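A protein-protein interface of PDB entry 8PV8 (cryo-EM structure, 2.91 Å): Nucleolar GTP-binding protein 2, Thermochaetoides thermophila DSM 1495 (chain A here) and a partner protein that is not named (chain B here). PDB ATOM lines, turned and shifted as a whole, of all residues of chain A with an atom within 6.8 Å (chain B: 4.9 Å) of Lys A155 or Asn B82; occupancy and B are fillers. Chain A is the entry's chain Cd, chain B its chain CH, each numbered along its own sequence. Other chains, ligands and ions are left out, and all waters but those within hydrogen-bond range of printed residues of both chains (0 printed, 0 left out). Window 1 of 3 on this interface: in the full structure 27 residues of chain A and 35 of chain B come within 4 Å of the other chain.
The backbone carbonyl oxygen of Asn B82 is in hydrogen-bond range of the guanidinium group of Arg A151, 3.4 Å away. NH2 of Arg A151 lies within hydrogen-bond range of O of Ile B83. The guanidinium group (NH1) of Arg A151 is in hydrogen-bond range of the backbone carbonyl oxygen (O) of Leu B84, at 2.7 Å. The side-chain amino group (NZ) of Lys A155 is in salt-bridge range of the side-chain carboxylate (OD2) of Asp B88.
The guanidinium group of Arg B78 lies within salt-bridge range of the side-chain carboxylate of Asp B79, 3.96 Å away.
Asp B86 touches Glu A139. Tyr B85 touches Arg A151. N of Asp B86 touches CZ of Arg A151, 3.9 Å away. Ile B83 touches Pro A154 (CD1 to CB, 3.97 Å). Lys A155 touches Asn B82. Leu A156 touches Ile B83 (CD2 to CD1, 3.97 Å). Asp B79 touches Tyr A167 (OD2 to CE1, 3.6 Å).
Of the printed residues of chain B, Arg A151 touches Asn B82, Ile B83, Leu B84, Tyr B85 and Asp B86. Lys A155 touches two residues of chain B. Arg B78 touches none of the printed residues of chain A. Leu B80 touches none of the printed residues of chain A. Printed residues of chain A within 4 Å of Asn B82: Arg A151 (3.4 Å) and Lys A155 (3.5 Å). Printed residues of chain A within 4 Å of Asp B86: Glu A139 (3.6 Å) and Arg A151 (3.9 Å). The nearest residue of chain B that does not touch Lys A155 is Asp B86 (4.3 Å). The nearest printed residue of chain B that does not touch Leu A156 is Asn B82 (4.8 Å).
Hydrophobic or aromatic side chains of chain B within 4 Å of the printed part of chain A: Ile B83. Along chain B the printed residues that touch a printed residue of chain A span positions 79 to 88. Of the 10 printed residues of chain A, 6 touch a printed residue of chain B. Among the printed residues, Asp or Glu carboxylates within 4 Å of a Lys or Arg side-chain nitrogen of the other chain: Lys A155 with Asp B88.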
ATOM      1  N   THR A 135      11.269  13.951  17.421  1.00  0.00           N
ATOM      2  CA  THR A 135      10.329  14.103  18.530  1.00  0.00           C
ATOM      3  C   THR A 135      11.053  14.406  19.836  1.00  0.00           C
ATOM      4  O   THR A 135      10.608  15.254  20.618  1.00  0.00           O
ATOM      5  CB  THR A 135       9.465  12.850  18.680  1.00  0.00           C
ATOM      6  OG1 THR A 135      10.291  11.683  18.608  1.00  0.00           O
ATOM      7  CG2 THR A 135       8.407  12.796  17.591  1.00  0.00           C
ATOM      8  N   GLU A 139      10.512  17.834  21.924  1.00  0.00           N
ATOM      9  CA  GLU A 139      10.054  17.694  23.304  1.00  0.00           C
ATOM     10  C   GLU A 139      11.019  16.781  24.045  1.00  0.00           C
ATOM     11  O   GLU A 139      11.036  15.562  23.800  1.00  0.00           O
ATOM     12  CB  GLU A 139       8.634  17.142  23.366  1.00  0.00           C
ATOM     13  CG  GLU A 139       7.701  17.689  22.297  1.00  0.00           C
ATOM     14  CD  GLU A 139       6.357  16.989  22.279  1.00  0.00           C
ATOM     15  OE1 GLU A 139       6.093  16.183  23.196  1.00  0.00           O
ATOM     16  OE2 GLU A 139       5.564  17.244  21.349  1.00  0.00           O
ATOM     17  N   ARG A 151       4.709  19.822  30.080  1.00  0.00           N
ATOM     18  CA  ARG A 151       3.694  19.343  29.152  1.00  0.00           C
ATOM     19  C   ARG A 151       2.310  19.460  29.775  1.00  0.00           C
ATOM     20  O   ARG A 151       2.083  19.009  30.901  1.00  0.00           O
ATOM     21  CB  ARG A 151       3.981  17.893  28.763  1.00  0.00           C
ATOM     22  CG  ARG A 151       2.789  17.147  28.188  1.00  0.00           C
ATOM     23  CD  ARG A 151       3.176  15.744  27.770  1.00  0.00           C
ATOM     24  NE  ARG A 151       2.026  14.973  27.317  1.00  0.00           N
ATOM     25  CZ  ARG A 151       1.353  14.121  28.078  1.00  0.00           C
ATOM     26  NH1 ARG A 151       1.688  13.907  29.338  1.00  0.00           N
ATOM     27  NH2 ARG A 151       0.317  13.468  27.560  1.00  0.00           N
ATOM     28  N   ARG A 153      -0.698  19.532  27.276  1.00  0.00           N
ATOM     29  CA  ARG A 153      -1.675  19.140  26.267  1.00  0.00           C
ATOM     30  C   ARG A 153      -1.313  17.769  25.716  1.00  0.00           C
ATOM     31  O   ARG A 153      -0.214  17.603  25.160  1.00  0.00           O
ATOM     32  CB  ARG A 153      -1.733  20.170  25.138  1.00  0.00           C
ATOM     33  CG  ARG A 153      -2.993  21.016  25.133  1.00  0.00           C
ATOM     34  CD  ARG A 153      -3.056  21.902  26.365  1.00  0.00           C
ATOM     35  NE  ARG A 153      -4.157  22.856  26.302  1.00  0.00           N
ATOM     36  CZ  ARG A 153      -4.439  23.738  27.251  1.00  0.00           C
ATOM     37  NH1 ARG A 153      -3.719  23.813  28.359  1.00  0.00           N
ATOM     38  NH2 ARG A 153      -5.466  24.564  27.085  1.00  0.00           N
ATOM     39  N   PRO A 154      -2.179  16.767  25.844  1.00  0.00           N
ATOM     40  CA  PRO A 154      -1.866  15.446  25.293  1.00  0.00           C
ATOM     41  C   PRO A 154      -1.974  15.435  23.776  1.00  0.00           C
ATOM     42  O   PRO A 154      -2.629  16.279  23.160  1.00  0.00           O
ATOM     43  CB  PRO A 154      -2.922  14.540  25.930  1.00  0.00           C
ATOM     44  CG  PRO A 154      -4.079  15.447  26.163  1.00  0.00           C
ATOM     45  CD  PRO A 154      -3.495  16.794  26.503  1.00  0.00           C
ATOM     46  N   LYS A 155      -1.311  14.451  23.174  1.00  0.00           N
ATOM     47  CA  LYS A 155      -1.363  14.237  21.731  1.00  0.00           C
ATOM     48  C   LYS A 155      -2.488  13.246  21.457  1.00  0.00           C
ATOM     49  O   LYS A 155      -2.378  12.058  21.772  1.00  0.00           O
ATOM     50  CB  LYS A 155      -0.026  13.732  21.200  1.00  0.00           C
ATOM     51  CG  LYS A 155       0.004  13.559  19.693  1.00  0.00           C
ATOM     52  CD  LYS A 155       1.346  13.033  19.221  1.00  0.00           C
ATOM     53  CE  LYS A 155       1.317  12.708  17.738  1.00  0.00           C
ATOM     54  NZ  LYS A 155       2.611  12.147  17.267  1.00  0.00           N
ATOM     55  N   LEU A 156      -3.572  13.738  20.870  1.00  0.00           N
ATOM     56  CA  LEU A 156      -4.779  12.955  20.670  1.00  0.00           C
ATOM     57  C   LEU A 156      -4.905  12.507  19.219  1.00  0.00           C
ATOM     58  O   LEU A 156      -4.403  13.151  18.295  1.00  0.00           O
ATOM     59  CB  LEU A 156      -6.013  13.765  21.070  1.00  0.00           C
ATOM     60  CG  LEU A 156      -6.092  14.199  22.533  1.00  0.00           C
ATOM     61  CD1 LEU A 156      -7.324  15.056  22.762  1.00  0.00           C
ATOM     62  CD2 LEU A 156      -6.085  12.993  23.457  1.00  0.00           C
ATOM     63  N   SER A 157      -5.593  11.381  19.033  1.00  0.00           N
ATOM     64  CA  SER A 157      -5.937  10.868  17.714  1.00  0.00           C
ATOM     65  C   SER A 157      -7.362  11.231  17.316  1.00  0.00           C
ATOM     66  O   SER A 157      -7.887  10.692  16.337  1.00  0.00           O
ATOM     67  CB  SER A 157      -5.745   9.352  17.672  1.00  0.00           C
ATOM     68  OG  SER A 157      -4.442   8.991  18.091  1.00  0.00           O
ATOM     69  N   PHE A 158      -7.994  12.134  18.062  1.00  0.00           N
ATOM     70  CA  PHE A 158      -9.392  12.493  17.880  1.00  0.00           C
ATOM     71  C   PHE A 158      -9.586  13.966  18.206  1.00  0.00           C
ATOM     72  O   PHE A 158      -8.839  14.537  19.005  1.00  0.00           O
ATOM     73  CB  PHE A 158     -10.297  11.601  18.752  1.00  0.00           C
ATOM     74  CG  PHE A 158     -10.066  11.756  20.234  1.00  0.00           C
ATOM     75  CD1 PHE A 158      -9.132  10.960  20.879  1.00  0.00           C
ATOM     76  CD2 PHE A 158     -10.789  12.671  20.986  1.00  0.00           C
ATOM     77  CE1 PHE A 158      -8.909  11.085  22.236  1.00  0.00           C
ATOM     78  CE2 PHE A 158     -10.567  12.801  22.344  1.00  0.00           C
ATOM     79  CZ  PHE A 158      -9.626  12.007  22.968  1.00  0.00           C
ATOM     80  N   TYR A 167     -13.509   6.062  18.133  1.00  0.00           N
ATOM     81  CA  TYR A 167     -12.175   5.561  18.452  1.00  0.00           C
ATOM     82  C   TYR A 167     -12.228   4.529  19.570  1.00  0.00           C
ATOM     83  O   TYR A 167     -11.559   3.493  19.501  1.00  0.00           O
ATOM     84  CB  TYR A 167     -11.267   6.731  18.834  1.00  0.00           C
ATOM     85  CG  TYR A 167      -9.816   6.368  19.057  1.00  0.00           C
ATOM     86  CD1 TYR A 167      -9.339   6.081  20.331  1.00  0.00           C
ATOM     87  CD2 TYR A 167      -8.922   6.322  17.996  1.00  0.00           C
ATOM     88  CE1 TYR A 167      -8.015   5.752  20.541  1.00  0.00           C
ATOM     89  CE2 TYR A 167      -7.593   5.993  18.196  1.00  0.00           C
ATOM     90  CZ  TYR A 167      -7.146   5.710  19.470  1.00  0.00           C
ATOM     91  OH  TYR A 167      -5.826   5.382  19.676  1.00  0.00           O
ATOM     92  N   ARG B  78      -4.519   1.747  27.950  1.00  0.00           N
ATOM     93  CA  ARG B  78      -3.640   2.306  26.926  1.00  0.00           C
ATOM     94  C   ARG B  78      -3.839   3.808  26.777  1.00  0.00           C
ATOM     95  O   ARG B  78      -2.869   4.575  26.760  1.00  0.00           O
ATOM     96  CB  ARG B  78      -3.892   1.613  25.588  1.00  0.00           C
ATOM     97  CG  ARG B  78      -3.160   2.248  24.416  1.00  0.00           C
ATOM     98  CD  ARG B  78      -3.195   1.351  23.196  1.00  0.00           C
ATOM     99  NE  ARG B  78      -4.460   1.461  22.482  1.00  0.00           N
ATOM    100  CZ  ARG B  78      -5.229   0.430  22.158  1.00  0.00           C
ATOM    101  NH1 ARG B  78      -4.896  -0.808  22.480  1.00  0.00           N
ATOM    102  NH2 ARG B  78      -6.362   0.649  21.498  1.00  0.00           N
ATOM    103  N   ASP B  79      -5.091   4.252  26.704  1.00  0.00           N
ATOM    104  CA  ASP B  79      -5.328   5.677  26.527  1.00  0.00           C
ATOM    105  C   ASP B  79      -5.094   6.459  27.815  1.00  0.00           C
ATOM    106  O   ASP B  79      -4.753   7.639  27.755  1.00  0.00           O
ATOM    107  CB  ASP B  79      -6.729   5.904  25.969  1.00  0.00           C
ATOM    108  CG  ASP B  79      -6.903   5.286  24.594  1.00  0.00           C
ATOM    109  OD1 ASP B  79      -5.894   4.813  24.031  1.00  0.00           O
ATOM    110  OD2 ASP B  79      -8.034   5.270  24.071  1.00  0.00           O
ATOM    111  N   LEU B  80      -5.230   5.826  28.982  1.00  0.00           N
ATOM    112  CA  LEU B  80      -4.848   6.490  30.226  1.00  0.00           C
ATOM    113  C   LEU B  80      -3.342   6.705  30.289  1.00  0.00           C
ATOM    114  O   LEU B  80      -2.871   7.759  30.737  1.00  0.00           O
ATOM    115  CB  LEU B  80      -5.327   5.675  31.426  1.00  0.00           C
ATOM    116  CG  LEU B  80      -5.044   6.275  32.804  1.00  0.00           C
ATOM    117  CD1 LEU B  80      -5.711   7.633  32.948  1.00  0.00           C
ATOM    118  CD2 LEU B  80      -5.491   5.332  33.907  1.00  0.00           C
ATOM    119  N   MET B  81      -2.570   5.714  29.834  1.00  0.00           N
ATOM    120  CA  MET B  81      -1.125   5.888  29.733  1.00  0.00           C
ATOM    121  C   MET B  81      -0.771   6.932  28.680  1.00  0.00           C
ATOM    122  O   MET B  81       0.242   7.627  28.805  1.00  0.00           O
ATOM    123  CB  MET B  81      -0.460   4.550  29.416  1.00  0.00           C
ATOM    124  CG  MET B  81      -0.559   3.537  30.541  1.00  0.00           C
ATOM    125  SD  MET B  81       0.221   1.967  30.139  1.00  0.00           S
ATOM    126  CE  MET B  81      -0.168   1.017  31.605  1.00  0.00           C
ATOM    127  N   ASN B  82      -1.592   7.051  27.634  1.00  0.00           N
ATOM    128  CA  ASN B  82      -1.369   8.086  26.626  1.00  0.00           C
ATOM    129  C   ASN B  82      -1.695   9.474  27.175  1.00  0.00           C
ATOM    130  O   ASN B  82      -1.091  10.474  26.772  1.00  0.00           O
ATOM    131  CB  ASN B  82      -2.202   7.793  25.377  1.00  0.00           C
ATOM    132  CG  ASN B  82      -2.040   8.856  24.305  1.00  0.00           C
ATOM    133  OD1 ASN B  82      -0.955   9.405  24.121  1.00  0.00           O
ATOM    134  ND2 ASN B  82      -3.125   9.162  23.605  1.00  0.00           N
ATOM    135  N   ILE B  83      -2.685   9.566  28.061  1.00  0.00           N
ATOM    136  CA  ILE B  83      -3.012  10.855  28.667  1.00  0.00           C
ATOM    137  C   ILE B  83      -1.926  11.276  29.651  1.00  0.00           C
ATOM    138  O   ILE B  83      -1.464  12.424  29.634  1.00  0.00           O
ATOM    139  CB  ILE B  83      -4.404  10.812  29.325  1.00  0.00           C
ATOM    140  CG1 ILE B  83      -5.481  10.662  28.251  1.00  0.00           C
ATOM    141  CG2 ILE B  83      -4.654  12.044  30.171  1.00  0.00           C
ATOM    142  CD1 ILE B  83      -5.423  11.712  27.157  1.00  0.00           C
ATOM    143  N   LEU B  84      -1.489  10.352  30.510  1.00  0.00           N
ATOM    144  CA  LEU B  84      -0.460  10.683  31.493  1.00  0.00           C
ATOM    145  C   LEU B  84       0.873  10.968  30.819  1.00  0.00           C
ATOM    146  O   LEU B  84       1.586  11.910  31.183  1.00  0.00           O
ATOM    147  CB  LEU B  84      -0.303   9.539  32.492  1.00  0.00           C
ATOM    148  CG  LEU B  84      -1.474   9.250  33.422  1.00  0.00           C
ATOM    149  CD1 LEU B  84      -1.288   7.901  34.089  1.00  0.00           C
ATOM    150  CD2 LEU B  84      -1.582  10.348  34.457  1.00  0.00           C
ATOM    151  N   TYR B  85       1.220  10.152  29.829  1.00  0.00           N
ATOM    152  CA  TYR B  85       2.550  10.061  29.246  1.00  0.00           C
ATOM    153  C   TYR B  85       2.410  10.202  27.744  1.00  0.00           C
ATOM    154  O   TYR B  85       1.484   9.634  27.162  1.00  0.00           O
ATOM    155  CB  TYR B  85       3.160   8.699  29.558  1.00  0.00           C
ATOM    156  CG  TYR B  85       3.496   8.462  30.998  1.00  0.00           C
ATOM    157  CD1 TYR B  85       3.573   9.506  31.907  1.00  0.00           C
ATOM    158  CD2 TYR B  85       3.627   7.177  31.469  1.00  0.00           C
ATOM    159  CE1 TYR B  85       3.857   9.269  33.216  1.00  0.00           C
ATOM    160  CE2 TYR B  85       3.875   6.945  32.764  1.00  0.00           C
ATOM    161  CZ  TYR B  85       4.001   7.978  33.634  1.00  0.00           C
ATOM    162  OH  TYR B  85       4.281   7.674  34.926  1.00  0.00           O
ATOM    163  N   ASP B  86       3.327  10.921  27.105  1.00  0.00           N
ATOM    164  CA  ASP B  86       3.362  10.864  25.650  1.00  0.00           C
ATOM    165  C   ASP B  86       3.765   9.457  25.225  1.00  0.00           C
ATOM    166  O   ASP B  86       4.872   9.000  25.525  1.00  0.00           O
ATOM    167  CB  ASP B  86       4.334  11.902  25.083  1.00  0.00           C
ATOM    168  CG  ASP B  86       4.177  12.087  23.576  1.00  0.00           C
ATOM    169  OD1 ASP B  86       3.183  11.585  23.016  1.00  0.00           O
ATOM    170  OD2 ASP B  86       5.038  12.742  22.951  1.00  0.00           O
ATOM    171  N   ALA B  87       2.829   8.754  24.572  1.00  0.00           N
ATOM    172  CA  ALA B  87       3.061   7.359  24.201  1.00  0.00           C
ATOM    173  C   ALA B  87       4.207   7.237  23.209  1.00  0.00           C
ATOM    174  O   ALA B  87       4.933   6.235  23.206  1.00  0.00           O
ATOM    175  CB  ALA B  87       1.788   6.746  23.622  1.00  0.00           C
ATOM    176  N   ASP B  88       4.385   8.256  22.367  1.00  0.00           N
ATOM    177  CA  ASP B  88       5.554   8.320  21.503  1.00  0.00           C
ATOM    178  C   ASP B  88       6.836   8.346  22.325  1.00  0.00           C
ATOM    179  O   ASP B  88       7.783   7.614  22.031  1.00  0.00           O
ATOM    180  CB  ASP B  88       5.465   9.550  20.601  1.00  0.00           C
ATOM    181  CG  ASP B  88       4.128   9.659  19.895  1.00  0.00           C
ATOM    182  OD1 ASP B  88       3.388   8.652  19.856  1.00  0.00           O
ATOM    183  OD2 ASP B  88       3.821  10.747  19.365  1.00  0.00           O
